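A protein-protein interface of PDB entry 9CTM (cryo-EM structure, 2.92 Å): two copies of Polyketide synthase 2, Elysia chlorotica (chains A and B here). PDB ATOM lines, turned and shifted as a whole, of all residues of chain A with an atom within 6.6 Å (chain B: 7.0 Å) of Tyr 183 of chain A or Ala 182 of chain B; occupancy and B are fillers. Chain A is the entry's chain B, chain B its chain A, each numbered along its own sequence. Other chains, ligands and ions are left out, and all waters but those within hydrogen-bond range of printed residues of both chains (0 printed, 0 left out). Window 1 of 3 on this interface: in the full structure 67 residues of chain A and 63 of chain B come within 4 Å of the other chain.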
ATOM      1  N   VAL A 133      -1.192 -20.713 -15.914  1.00  0.00           N
ATOM      2  CA  VAL A 133      -0.389 -21.875 -16.277  1.00  0.00           C
ATOM      3  C   VAL A 133       0.127 -22.507 -14.993  1.00  0.00           C
ATOM      4  O   VAL A 133       0.622 -21.806 -14.104  1.00  0.00           O
ATOM      5  CB  VAL A 133       0.770 -21.495 -17.214  1.00  0.00           C
ATOM      6  CG1 VAL A 133       1.267 -22.723 -17.958  1.00  0.00           C
ATOM      7  CG2 VAL A 133       0.333 -20.416 -18.192  1.00  0.00           C
ATOM      8  N   TYR A 134       0.007 -23.826 -14.896  1.00  0.00           N
ATOM      9  CA  TYR A 134       0.300 -24.581 -13.681  1.00  0.00           C
ATOM     10  C   TYR A 134       1.194 -25.769 -14.002  1.00  0.00           C
ATOM     11  O   TYR A 134       0.884 -26.918 -13.688  1.00  0.00           O
ATOM     12  CB  TYR A 134      -0.996 -25.022 -13.007  1.00  0.00           C
ATOM     13  CG  TYR A 134      -1.856 -23.856 -12.579  1.00  0.00           C
ATOM     14  CD1 TYR A 134      -1.538 -23.113 -11.451  1.00  0.00           C
ATOM     15  CD2 TYR A 134      -2.976 -23.489 -13.311  1.00  0.00           C
ATOM     16  CE1 TYR A 134      -2.316 -22.044 -11.057  1.00  0.00           C
ATOM     17  CE2 TYR A 134      -3.761 -22.419 -12.927  1.00  0.00           C
ATOM     18  CZ  TYR A 134      -3.425 -21.701 -11.799  1.00  0.00           C
ATOM     19  OH  TYR A 134      -4.202 -20.635 -11.411  1.00  0.00           O
ATOM     20  N   ILE A 135       2.316 -25.501 -14.672  1.00  0.00           N
ATOM     21  CA  ILE A 135       3.139 -26.593 -15.178  1.00  0.00           C
ATOM     22  C   ILE A 135       3.696 -27.406 -14.019  1.00  0.00           C
ATOM     23  O   ILE A 135       3.980 -26.875 -12.938  1.00  0.00           O
ATOM     24  CB  ILE A 135       4.270 -26.050 -16.069  1.00  0.00           C
ATOM     25  CG1 ILE A 135       3.697 -25.263 -17.251  1.00  0.00           C
ATOM     26  CG2 ILE A 135       5.148 -27.190 -16.566  1.00  0.00           C
ATOM     27  CD1 ILE A 135       2.682 -26.030 -18.081  1.00  0.00           C
ATOM     28  N   GLY A 136       3.824 -28.713 -14.235  1.00  0.00           N
ATOM     29  CA  GLY A 136       4.455 -29.593 -13.269  1.00  0.00           C
ATOM     30  C   GLY A 136       5.694 -30.254 -13.836  1.00  0.00           C
ATOM     31  O   GLY A 136       5.595 -31.101 -14.728  1.00  0.00           O
ATOM     32  N   VAL A 137       6.865 -29.881 -13.327  1.00  0.00           N
ATOM     33  CA  VAL A 137       8.135 -30.398 -13.822  1.00  0.00           C
ATOM     34  C   VAL A 137       9.101 -30.526 -12.653  1.00  0.00           C
ATOM     35  O   VAL A 137       9.136 -29.666 -11.765  1.00  0.00           O
ATOM     36  CB  VAL A 137       8.723 -29.491 -14.924  1.00  0.00           C
ATOM     37  CG1 VAL A 137       8.756 -28.039 -14.465  1.00  0.00           C
ATOM     38  CG2 VAL A 137      10.113 -29.964 -15.315  1.00  0.00           C
ATOM     39  N   SER A 138       9.885 -31.604 -12.655  1.00  0.00           N
ATOM     40  CA  SER A 138      10.851 -31.851 -11.590  1.00  0.00           C
ATOM     41  C   SER A 138      12.242 -32.120 -12.154  1.00  0.00           C
ATOM     42  O   SER A 138      13.247 -31.733 -11.547  1.00  0.00           O
ATOM     43  CB  SER A 138      10.399 -33.030 -10.726  1.00  0.00           C
ATOM     44  OG  SER A 138      11.038 -34.229 -11.126  1.00  0.00           O
ATOM     45  N   SER A 180       1.187 -17.804 -13.306  1.00  0.00           N
ATOM     46  CA  SER A 180       2.031 -18.800 -13.953  1.00  0.00           C
ATOM     47  C   SER A 180       2.963 -19.394 -12.906  1.00  0.00           C
ATOM     48  O   SER A 180       3.726 -18.664 -12.265  1.00  0.00           O
ATOM     49  CB  SER A 180       2.828 -18.178 -15.100  1.00  0.00           C
ATOM     50  OG  SER A 180       3.847 -17.323 -14.610  1.00  0.00           O
ATOM     51  N   THR A 181       2.905 -20.713 -12.737  1.00  0.00           N
ATOM     52  CA  THR A 181       3.646 -21.367 -11.670  1.00  0.00           C
ATOM     53  C   THR A 181       4.129 -22.735 -12.131  1.00  0.00           C
ATOM     54  O   THR A 181       3.536 -23.365 -13.015  1.00  0.00           O
ATOM     55  CB  THR A 181       2.790 -21.513 -10.405  1.00  0.00           C
ATOM     56  OG1 THR A 181       2.120 -20.277 -10.131  1.00  0.00           O
ATOM     57  CG2 THR A 181       3.654 -21.897  -9.211  1.00  0.00           C
ATOM     58  N   ALA A 182       5.233 -23.169 -11.527  1.00  0.00           N
ATOM     59  CA  ALA A 182       5.800 -24.493 -11.732  1.00  0.00           C
ATOM     60  C   ALA A 182       5.811 -25.224 -10.399  1.00  0.00           C
ATOM     61  O   ALA A 182       6.361 -24.719  -9.414  1.00  0.00           O
ATOM     62  CB  ALA A 182       7.217 -24.409 -12.307  1.00  0.00           C
ATOM     63  N   TYR A 183       5.206 -26.405 -10.372  1.00  0.00           N
ATOM     64  CA  TYR A 183       5.074 -27.200  -9.162  1.00  0.00           C
ATOM     65  C   TYR A 183       6.002 -28.405  -9.226  1.00  0.00           C
ATOM     66  O   TYR A 183       6.213 -28.993 -10.290  1.00  0.00           O
ATOM     67  CB  TYR A 183       3.631 -27.676  -8.967  1.00  0.00           C
ATOM     68  CG  TYR A 183       2.621 -26.562  -8.795  1.00  0.00           C
ATOM     69  CD1 TYR A 183       2.269 -25.743  -9.860  1.00  0.00           C
ATOM     70  CD2 TYR A 183       2.012 -26.336  -7.568  1.00  0.00           C
ATOM     71  CE1 TYR A 183       1.345 -24.728  -9.706  1.00  0.00           C
ATOM     72  CE2 TYR A 183       1.086 -25.323  -7.405  1.00  0.00           C
ATOM     73  CZ  TYR A 183       0.757 -24.521  -8.477  1.00  0.00           C
ATOM     74  OH  TYR A 183      -0.164 -23.511  -8.318  1.00  0.00           O
ATOM     75  N   ASN A 184       6.556 -28.767  -8.070  1.00  0.00           N
ATOM     76  CA  ASN A 184       7.413 -29.946  -7.948  1.00  0.00           C
ATOM     77  C   ASN A 184       6.942 -30.727  -6.726  1.00  0.00           C
ATOM     78  O   ASN A 184       7.362 -30.445  -5.600  1.00  0.00           O
ATOM     79  CB  ASN A 184       8.882 -29.562  -7.831  1.00  0.00           C
ATOM     80  CG  ASN A 184       9.801 -30.768  -7.843  1.00  0.00           C
ATOM     81  OD1 ASN A 184       9.343 -31.910  -7.884  1.00  0.00           O
ATOM     82  ND2 ASN A 184      11.103 -30.519  -7.812  1.00  0.00           N
ATOM     83  N   THR A 185       6.068 -31.705  -6.956  1.00  0.00           N
ATOM     84  CA  THR A 185       5.512 -32.540  -5.900  1.00  0.00           C
ATOM     85  C   THR A 185       5.833 -34.011  -6.143  1.00  0.00           C
ATOM     86  O   THR A 185       5.080 -34.895  -5.732  1.00  0.00           O
ATOM     87  CB  THR A 185       4.001 -32.331  -5.795  1.00  0.00           C
ATOM     88  OG1 THR A 185       3.697 -30.937  -5.933  1.00  0.00           O
ATOM     89  CG2 THR A 185       3.473 -32.831  -4.459  1.00  0.00           C
ATOM     90  N   ALA A 186       6.958 -34.284  -6.801  1.00  0.00           N
ATOM     91  CA  ALA A 186       7.284 -35.639  -7.229  1.00  0.00           C
ATOM     92  C   ALA A 186       6.126 -36.160  -8.070  1.00  0.00           C
ATOM     93  O   ALA A 186       5.583 -35.430  -8.898  1.00  0.00           O
ATOM     94  CB  ALA A 186       7.544 -36.541  -6.029  1.00  0.00           C
ATOM     95  N   THR A 189       2.296 -34.415  -8.969  1.00  0.00           N
ATOM     96  CA  THR A 189       2.464 -33.014  -9.345  1.00  0.00           C
ATOM     97  C   THR A 189       1.356 -32.563 -10.287  1.00  0.00           C
ATOM     98  O   THR A 189       0.841 -31.447 -10.159  1.00  0.00           O
ATOM     99  CB  THR A 189       3.833 -32.797  -9.990  1.00  0.00           C
ATOM    100  OG1 THR A 189       4.856 -33.335  -9.144  1.00  0.00           O
ATOM    101  CG2 THR A 189       4.095 -31.311 -10.210  1.00  0.00           C
ATOM    102  N   VAL A 192      -1.730 -32.033  -8.295  1.00  0.00           N
ATOM    103  CA  VAL A 192      -1.564 -30.836  -7.474  1.00  0.00           C
ATOM    104  C   VAL A 192      -1.793 -29.586  -8.313  1.00  0.00           C
ATOM    105  O   VAL A 192      -2.440 -28.628  -7.871  1.00  0.00           O
ATOM    106  CB  VAL A 192      -0.172 -30.833  -6.815  1.00  0.00           C
ATOM    107  CG1 VAL A 192       0.219 -29.425  -6.381  1.00  0.00           C
ATOM    108  CG2 VAL A 192      -0.143 -31.790  -5.634  1.00  0.00           C
ATOM    109  N   CYS A 193      -1.258 -29.571  -9.534  1.00  0.00           N
ATOM    110  CA  CYS A 193      -1.480 -28.444 -10.432  1.00  0.00           C
ATOM    111  C   CYS A 193      -2.951 -28.325 -10.806  1.00  0.00           C
ATOM    112  O   CYS A 193      -3.484 -27.215 -10.919  1.00  0.00           O
ATOM    113  CB  CYS A 193      -0.616 -28.600 -11.682  1.00  0.00           C
ATOM    114  SG  CYS A 193       1.158 -28.505 -11.356  1.00  0.00           S
ATOM    115  N   ALA A 196      -4.613 -26.694  -7.904  1.00  0.00           N
ATOM    116  CA  ALA A 196      -4.328 -25.261  -7.888  1.00  0.00           C
ATOM    117  C   ALA A 196      -5.155 -24.528  -8.937  1.00  0.00           C
ATOM    118  O   ALA A 196      -5.669 -23.430  -8.683  1.00  0.00           O
ATOM    119  CB  ALA A 196      -2.836 -25.022  -8.119  1.00  0.00           C
ATOM    120  N   ALA A 197      -5.288 -25.117 -10.127  1.00  0.00           N
ATOM    121  CA  ALA A 197      -6.103 -24.505 -11.170  1.00  0.00           C
ATOM    122  C   ALA A 197      -7.560 -24.412 -10.739  1.00  0.00           C
ATOM    123  O   ALA A 197      -8.227 -23.404 -10.997  1.00  0.00           O
ATOM    124  CB  ALA A 197      -5.979 -25.303 -12.467  1.00  0.00           C
ATOM    125  N   HIS A 200      -7.850 -21.533  -8.207  1.00  0.00           N
ATOM    126  CA  HIS A 200      -7.815 -20.212  -8.827  1.00  0.00           C
ATOM    127  C   HIS A 200      -9.049 -19.962  -9.687  1.00  0.00           C
ATOM    128  O   HIS A 200      -9.474 -18.812  -9.838  1.00  0.00           O
ATOM    129  CB  HIS A 200      -6.542 -20.059  -9.657  1.00  0.00           C
ATOM    130  CG  HIS A 200      -5.313 -19.811  -8.837  1.00  0.00           C
ATOM    131  ND1 HIS A 200      -4.749 -18.562  -8.702  1.00  0.00           N
ATOM    132  CD2 HIS A 200      -4.543 -20.652  -8.108  1.00  0.00           C
ATOM    133  CE1 HIS A 200      -3.682 -18.644  -7.926  1.00  0.00           C
ATOM    134  NE2 HIS A 200      -3.536 -19.902  -7.551  1.00  0.00           N
ATOM    135  N   THR A 359       7.015 -37.413 -12.285  1.00  0.00           N
ATOM    136  CA  THR A 359       6.349 -36.135 -12.058  1.00  0.00           C
ATOM    137  C   THR A 359       5.127 -35.969 -12.952  1.00  0.00           C
ATOM    138  O   THR A 359       4.140 -35.348 -12.543  1.00  0.00           O
ATOM    139  CB  THR A 359       7.328 -34.983 -12.288  1.00  0.00           C
ATOM    140  OG1 THR A 359       8.577 -35.275 -11.649  1.00  0.00           O
ATOM    141  CG2 THR A 359       6.768 -33.682 -11.728  1.00  0.00           C
ATOM    142  N   VAL B 133       2.223 -27.268   4.031  1.00  0.00           N
ATOM    143  CA  VAL B 133       3.567 -26.748   3.808  1.00  0.00           C
ATOM    144  C   VAL B 133       3.661 -26.304   2.355  1.00  0.00           C
ATOM    145  O   VAL B 133       3.223 -27.022   1.450  1.00  0.00           O
ATOM    146  CB  VAL B 133       4.644 -27.794   4.139  1.00  0.00           C
ATOM    147  CG1 VAL B 133       5.982 -27.114   4.378  1.00  0.00           C
ATOM    148  CG2 VAL B 133       4.235 -28.613   5.355  1.00  0.00           C
ATOM    149  N   TYR B 134       4.234 -25.125   2.136  1.00  0.00           N
ATOM    150  CA  TYR B 134       4.262 -24.467   0.834  1.00  0.00           C
ATOM    151  C   TYR B 134       5.665 -23.967   0.528  1.00  0.00           C
ATOM    152  O   TYR B 134       5.887 -22.792   0.235  1.00  0.00           O
ATOM    153  CB  TYR B 134       3.243 -23.334   0.791  1.00  0.00           C
ATOM    154  CG  TYR B 134       1.825 -23.814   0.983  1.00  0.00           C
ATOM    155  CD1 TYR B 134       1.143 -24.451  -0.044  1.00  0.00           C
ATOM    156  CD2 TYR B 134       1.173 -23.649   2.198  1.00  0.00           C
ATOM    157  CE1 TYR B 134      -0.151 -24.898   0.127  1.00  0.00           C
ATOM    158  CE2 TYR B 134      -0.122 -24.094   2.379  1.00  0.00           C
ATOM    159  CZ  TYR B 134      -0.779 -24.718   1.341  1.00  0.00           C
ATOM    160  OH  TYR B 134      -2.068 -25.164   1.515  1.00  0.00           O
ATOM    161  N   ILE B 135       6.647 -24.863   0.627  1.00  0.00           N
ATOM    162  CA  ILE B 135       8.038 -24.438   0.536  1.00  0.00           C
ATOM    163  C   ILE B 135       8.324 -23.879  -0.853  1.00  0.00           C
ATOM    164  O   ILE B 135       7.706 -24.273  -1.852  1.00  0.00           O
ATOM    165  CB  ILE B 135       8.988 -25.602   0.873  1.00  0.00           C
ATOM    166  CG1 ILE B 135       8.713 -26.133   2.283  1.00  0.00           C
ATOM    167  CG2 ILE B 135      10.440 -25.160   0.751  1.00  0.00           C
ATOM    168  CD1 ILE B 135       8.767 -25.076   3.373  1.00  0.00           C
ATOM    169  N   GLY B 136       9.255 -22.931  -0.913  1.00  0.00           N
ATOM    170  CA  GLY B 136       9.712 -22.382  -2.175  1.00  0.00           C
ATOM    171  C   GLY B 136      11.202 -22.580  -2.353  1.00  0.00           C
ATOM    172  O   GLY B 136      12.004 -21.978  -1.632  1.00  0.00           O
ATOM    173  N   VAL B 137      11.587 -23.419  -3.311  1.00  0.00           N
ATOM    174  CA  VAL B 137      12.983 -23.781  -3.521  1.00  0.00           C
ATOM    175  C   VAL B 137      13.203 -24.026  -5.007  1.00  0.00           C
ATOM    176  O   VAL B 137      12.370 -24.648  -5.675  1.00  0.00           O
ATOM    177  CB  VAL B 137      13.370 -25.023  -2.690  1.00  0.00           C
ATOM    178  CG1 VAL B 137      12.552 -26.236  -3.123  1.00  0.00           C
ATOM    179  CG2 VAL B 137      14.866 -25.302  -2.790  1.00  0.00           C
ATOM    180  N   HIS B 163      13.619 -31.729  -4.495  1.00  0.00           N
ATOM    181  CA  HIS B 163      12.944 -30.515  -4.057  1.00  0.00           C
ATOM    182  C   HIS B 163      11.526 -30.774  -3.566  1.00  0.00           C
ATOM    183  O   HIS B 163      10.993 -29.960  -2.805  1.00  0.00           O
ATOM    184  CB  HIS B 163      12.916 -29.494  -5.197  1.00  0.00           C
ATOM    185  CG  HIS B 163      14.154 -28.656  -5.291  1.00  0.00           C
ATOM    186  ND1 HIS B 163      14.598 -28.116  -6.478  1.00  0.00           N
ATOM    187  CD2 HIS B 163      15.042 -28.268  -4.346  1.00  0.00           C
ATOM    188  CE1 HIS B 163      15.706 -27.430  -6.261  1.00  0.00           C
ATOM    189  NE2 HIS B 163      15.997 -27.507  -4.976  1.00  0.00           N
ATOM    190  N   SER B 164      10.905 -31.880  -3.980  1.00  0.00           N
ATOM    191  CA  SER B 164       9.580 -32.217  -3.474  1.00  0.00           C
ATOM    192  C   SER B 164       9.625 -32.693  -2.030  1.00  0.00           C
ATOM    193  O   SER B 164       8.600 -32.648  -1.342  1.00  0.00           O
ATOM    194  CB  SER B 164       8.936 -33.292  -4.351  1.00  0.00           C
ATOM    195  OG  SER B 164       9.253 -34.589  -3.876  1.00  0.00           O
ATOM    196  N   MET B 165      10.785 -33.151  -1.558  1.00  0.00           N
ATOM    197  CA  MET B 165      10.923 -33.621  -0.187  1.00  0.00           C
ATOM    198  C   MET B 165      11.118 -32.488   0.811  1.00  0.00           C
ATOM    199  O   MET B 165      11.001 -32.726   2.018  1.00  0.00           O
ATOM    200  CB  MET B 165      12.101 -34.592  -0.085  1.00  0.00           C
ATOM    201  CG  MET B 165      11.993 -35.790  -1.014  1.00  0.00           C
ATOM    202  SD  MET B 165      10.573 -36.839  -0.650  1.00  0.00           S
ATOM    203  CE  MET B 165      11.069 -37.563   0.910  1.00  0.00           C
ATOM    204  N   TYR B 166      11.411 -31.274   0.348  1.00  0.00           N
ATOM    205  CA  TYR B 166      11.568 -30.154   1.274  1.00  0.00           C
ATOM    206  C   TYR B 166      10.315 -29.927   2.106  1.00  0.00           C
ATOM    207  O   TYR B 166      10.424 -29.849   3.342  1.00  0.00           O
ATOM    208  CB  TYR B 166      11.945 -28.890   0.496  1.00  0.00           C
ATOM    209  CG  TYR B 166      13.400 -28.824   0.090  1.00  0.00           C
ATOM    210  CD1 TYR B 166      14.014 -29.893  -0.548  1.00  0.00           C
ATOM    211  CD2 TYR B 166      14.158 -27.689   0.342  1.00  0.00           C
ATOM    212  CE1 TYR B 166      15.341 -29.835  -0.921  1.00  0.00           C
ATOM    213  CE2 TYR B 166      15.487 -27.622  -0.028  1.00  0.00           C
ATOM    214  CZ  TYR B 166      16.073 -28.697  -0.660  1.00  0.00           C
ATOM    215  OH  TYR B 166      17.394 -28.636  -1.031  1.00  0.00           O
ATOM    216  N   PRO B 167       9.120 -29.813   1.521  1.00  0.00           N
ATOM    217  CA  PRO B 167       7.918 -29.700   2.363  1.00  0.00           C
ATOM    218  C   PRO B 167       7.528 -31.013   3.013  1.00  0.00           C
ATOM    219  O   PRO B 167       7.164 -31.032   4.195  1.00  0.00           O
ATOM    220  CB  PRO B 167       6.851 -29.215   1.373  1.00  0.00           C
ATOM    221  CG  PRO B 167       7.308 -29.745   0.058  1.00  0.00           C
ATOM    222  CD  PRO B 167       8.805 -29.691   0.087  1.00  0.00           C
ATOM    223  N   ASN B 168       7.610 -32.121   2.271  1.00  0.00           N
ATOM    224  CA  ASN B 168       7.163 -33.406   2.796  1.00  0.00           C
ATOM    225  C   ASN B 168       7.883 -33.746   4.094  1.00  0.00           C
ATOM    226  O   ASN B 168       7.255 -34.149   5.079  1.00  0.00           O
ATOM    227  CB  ASN B 168       7.385 -34.496   1.748  1.00  0.00           C
ATOM    228  CG  ASN B 168       6.575 -34.266   0.487  1.00  0.00           C
ATOM    229  OD1 ASN B 168       5.815 -33.301   0.392  1.00  0.00           O
ATOM    230  ND2 ASN B 168       6.738 -35.146  -0.492  1.00  0.00           N
ATOM    231  N   SER B 180       1.204 -30.556   1.070  1.00  0.00           N
ATOM    232  CA  SER B 180       2.629 -30.251   1.102  1.00  0.00           C
ATOM    233  C   SER B 180       3.115 -30.100  -0.332  1.00  0.00           C
ATOM    234  O   SER B 180       2.963 -31.021  -1.141  1.00  0.00           O
ATOM    235  CB  SER B 180       3.407 -31.349   1.829  1.00  0.00           C
ATOM    236  OG  SER B 180       3.485 -32.527   1.046  1.00  0.00           O
ATOM    237  N   THR B 181       3.695 -28.943  -0.644  1.00  0.00           N
ATOM    238  CA  THR B 181       4.066 -28.630  -2.014  1.00  0.00           C
ATOM    239  C   THR B 181       5.326 -27.776  -2.037  1.00  0.00           C
ATOM    240  O   THR B 181       5.648 -27.075  -1.069  1.00  0.00           O
ATOM    241  CB  THR B 181       2.929 -27.902  -2.746  1.00  0.00           C
ATOM    242  OG1 THR B 181       1.676 -28.518  -2.421  1.00  0.00           O
ATOM    243  CG2 THR B 181       3.139 -27.954  -4.253  1.00  0.00           C
ATOM    244  N   ALA B 182       6.042 -27.865  -3.156  1.00  0.00           N
ATOM    245  CA  ALA B 182       7.221 -27.058  -3.431  1.00  0.00           C
ATOM    246  C   ALA B 182       6.967 -26.251  -4.695  1.00  0.00           C
ATOM    247  O   ALA B 182       6.537 -26.805  -5.712  1.00  0.00           O
ATOM    248  CB  ALA B 182       8.467 -27.933  -3.596  1.00  0.00           C
ATOM    249  N   TYR B 183       7.233 -24.952  -4.629  1.00  0.00           N
ATOM    250  CA  TYR B 183       6.934 -24.032  -5.715  1.00  0.00           C
ATOM    251  C   TYR B 183       8.218 -23.481  -6.321  1.00  0.00           C
ATOM    252  O   TYR B 183       9.248 -23.360  -5.652  1.00  0.00           O
ATOM    253  CB  TYR B 183       6.063 -22.869  -5.225  1.00  0.00           C
ATOM    254  CG  TYR B 183       4.685 -23.277  -4.752  1.00  0.00           C
ATOM    255  CD1 TYR B 183       4.512 -23.946  -3.547  1.00  0.00           C
ATOM    256  CD2 TYR B 183       3.556 -22.982  -5.504  1.00  0.00           C
ATOM    257  CE1 TYR B 183       3.255 -24.315  -3.109  1.00  0.00           C
ATOM    258  CE2 TYR B 183       2.296 -23.347  -5.073  1.00  0.00           C
ATOM    259  CZ  TYR B 183       2.150 -24.014  -3.876  1.00  0.00           C
ATOM    260  OH  TYR B 183       0.896 -24.379  -3.446  1.00  0.00           O
ATOM    261  N   ASN B 184       8.140 -23.146  -7.609  1.00  0.00           N
ATOM    262  CA  ASN B 184       9.234 -22.455  -8.288  1.00  0.00           C
ATOM    263  C   ASN B 184       8.611 -21.474  -9.276  1.00  0.00           C
ATOM    264  O   ASN B 184       8.265 -21.856 -10.398  1.00  0.00           O
ATOM    265  CB  ASN B 184      10.171 -23.427  -8.990  1.00  0.00           C
ATOM    266  CG  ASN B 184      11.348 -22.725  -9.642  1.00  0.00           C
ATOM    267  OD1 ASN B 184      11.523 -21.515  -9.492  1.00  0.00           O
ATOM    268  ND2 ASN B 184      12.163 -23.478 -10.369  1.00  0.00           N
ATOM    269  N   THR B 189       8.486 -16.447  -5.891  1.00  0.00           N
ATOM    270  CA  THR B 189       8.034 -17.759  -5.437  1.00  0.00           C
ATOM    271  C   THR B 189       7.478 -17.718  -4.018  1.00  0.00           C
ATOM    272  O   THR B 189       6.466 -18.369  -3.739  1.00  0.00           O
ATOM    273  CB  THR B 189       9.178 -18.768  -5.516  1.00  0.00           C
ATOM    274  OG1 THR B 189       9.887 -18.602  -6.751  1.00  0.00           O
ATOM    275  CG2 THR B 189       8.641 -20.191  -5.428  1.00  0.00           C
ATOM    276  N   VAL B 192       4.118 -16.343  -3.938  1.00  0.00           N
ATOM    277  CA  VAL B 192       3.248 -17.330  -4.576  1.00  0.00           C
ATOM    278  C   VAL B 192       2.844 -18.402  -3.570  1.00  0.00           C
ATOM    279  O   VAL B 192       1.682 -18.826  -3.518  1.00  0.00           O
ATOM    280  CB  VAL B 192       3.950 -17.938  -5.805  1.00  0.00           C
ATOM    281  CG1 VAL B 192       3.332 -19.281  -6.172  1.00  0.00           C
ATOM    282  CG2 VAL B 192       3.887 -16.975  -6.979  1.00  0.00           C
ATOM    283  N   CYS B 193       3.801 -18.863  -2.762  1.00  0.00           N
ATOM    284  CA  CYS B 193       3.488 -19.829  -1.713  1.00  0.00           C
ATOM    285  C   CYS B 193       2.536 -19.228  -0.688  1.00  0.00           C
ATOM    286  O   CYS B 193       1.628 -19.908  -0.196  1.00  0.00           O
ATOM    287  CB  CYS B 193       4.777 -20.295  -1.040  1.00  0.00           C
ATOM    288  SG  CYS B 193       5.878 -21.223  -2.129  1.00  0.00           S
ATOM    289  N   ALA B 196      -0.869 -19.353  -2.220  1.00  0.00           N
ATOM    290  CA  ALA B 196      -1.410 -20.708  -2.171  1.00  0.00           C
ATOM    291  C   ALA B 196      -1.895 -21.053  -0.768  1.00  0.00           C
ATOM    292  O   ALA B 196      -2.951 -21.676  -0.598  1.00  0.00           O
ATOM    293  CB  ALA B 196      -0.355 -21.711  -2.636  1.00  0.00           C
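Thr 181 of chain A touches Tyr 183 of chain B, and with the chains exchanged Tyr 183 of chain A touches Thr 181 of chain B.
Ala 182 of chain A touches Tyr 183 of chain B, and with the chains exchanged Tyr 183 of chain A touches Ala 182 of chain B.
Tyr 183 of chain A touches its own counterpart, Tyr 183 of chain B.
Val 192 of chain A touches Thr 181 of chain B, but with the chains exchanged Thr 181 of chain A does not touch Val 192 of chain B (4.02 Å).
Positions printed for both chains: 133, 134, 135, 136, 137, 180, 181, 182, 183, 184, 189, 192, 193 and 196.
Of chain B, only Thr 181, Ala 182 and Tyr 183 come within 4 Å of Tyr 183 of chain A.
Ala 182 of chain B touches just these residues of chain A: Tyr 183 and Asn 184.
Printed residues of chain A within 4 Å of Thr 181 of chain B: Tyr 183, Thr 185 and Val 192.
Of the printed residues of chain A, Asn 184 of chain B touches Ala 182.
Printed residues of chain A within 4 Å of Tyr 183 of chain B: Thr 181 (3.9 Å), Ala 182 (3.8 Å) and Tyr 183 (3.3 Å).
The nearest residue of chain A that does not touch Ala 182 of chain B is Ala 182 of chain A (4.3 Å).
O of Val 133 of chain B lies within hydrogen-bond range of N of Thr 181 of chain B (2.9 Å).
The backbone NH of Val 137 of chain B sits at hydrogen-bond distance from the backbone carbonyl oxygen of Tyr 183 of chain B.
N of Thr 181 of chain A lies within hydrogen-bond range of O of Val 133 of chain A.
The backbone carbonyl oxygen (O) of Ile 135 of chain A is in hydrogen-bond range of the backbone NH (N) of Tyr 183 of chain A (2.9 Å).
O of Tyr 183 of chain A lies within hydrogen-bond range of N of Val 137 of chain A.
The side-chain hydroxyl (OG1) of Thr 189 of chain A sits at hydrogen-bond distance from the backbone NH (N) of Thr 185 of chain A, 3.0 Å away.
The backbone NH of Asn 184 of chain A is in hydrogen-bond range of the backbone carbonyl oxygen of Ala 182 of chain B (3.1 Å).
O of Ala 182 of chain A is in hydrogen-bond range of N of Asn 184 of chain B (3.0 Å).
Among the printed residues, pairs that only touch across the chains: Tyr 183 of chain A with Tyr 183 of chain B, Ala 186 of chain A with Ser 164 of chain B, Asn 184 of chain A with His 163 of chain B, Thr 185 of chain A with Thr 181 of chain B, Asn 184 of chain A with Ser 164 of chain B, Thr 185 of chain A with Ser 164 of chain B, Tyr 183 of chain A with Ala 182 of chain B, Ala 182 of chain A with Tyr 183 of chain B, Thr 185 of chain A with Ser 180 of chain B, Tyr 183 of chain A with Thr 181 of chain B, Thr 181 of chain A with Tyr 183 of chain B and Val 192 of chain A with Thr 181 of chain B.
Of the 20 printed residues of chain B, 7 touch a printed residue of chain A.
Printed residues of chain A that touch a printed residue of chain B: Thr 181, Ala 182, Tyr 183, Asn 184, Thr 185, Ala 186 and Val 192.
Hydrophobic or aromatic side chains of chain A that line the printed part of chain B: Ala 182, Tyr 183, Ala 186 and Val 192.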
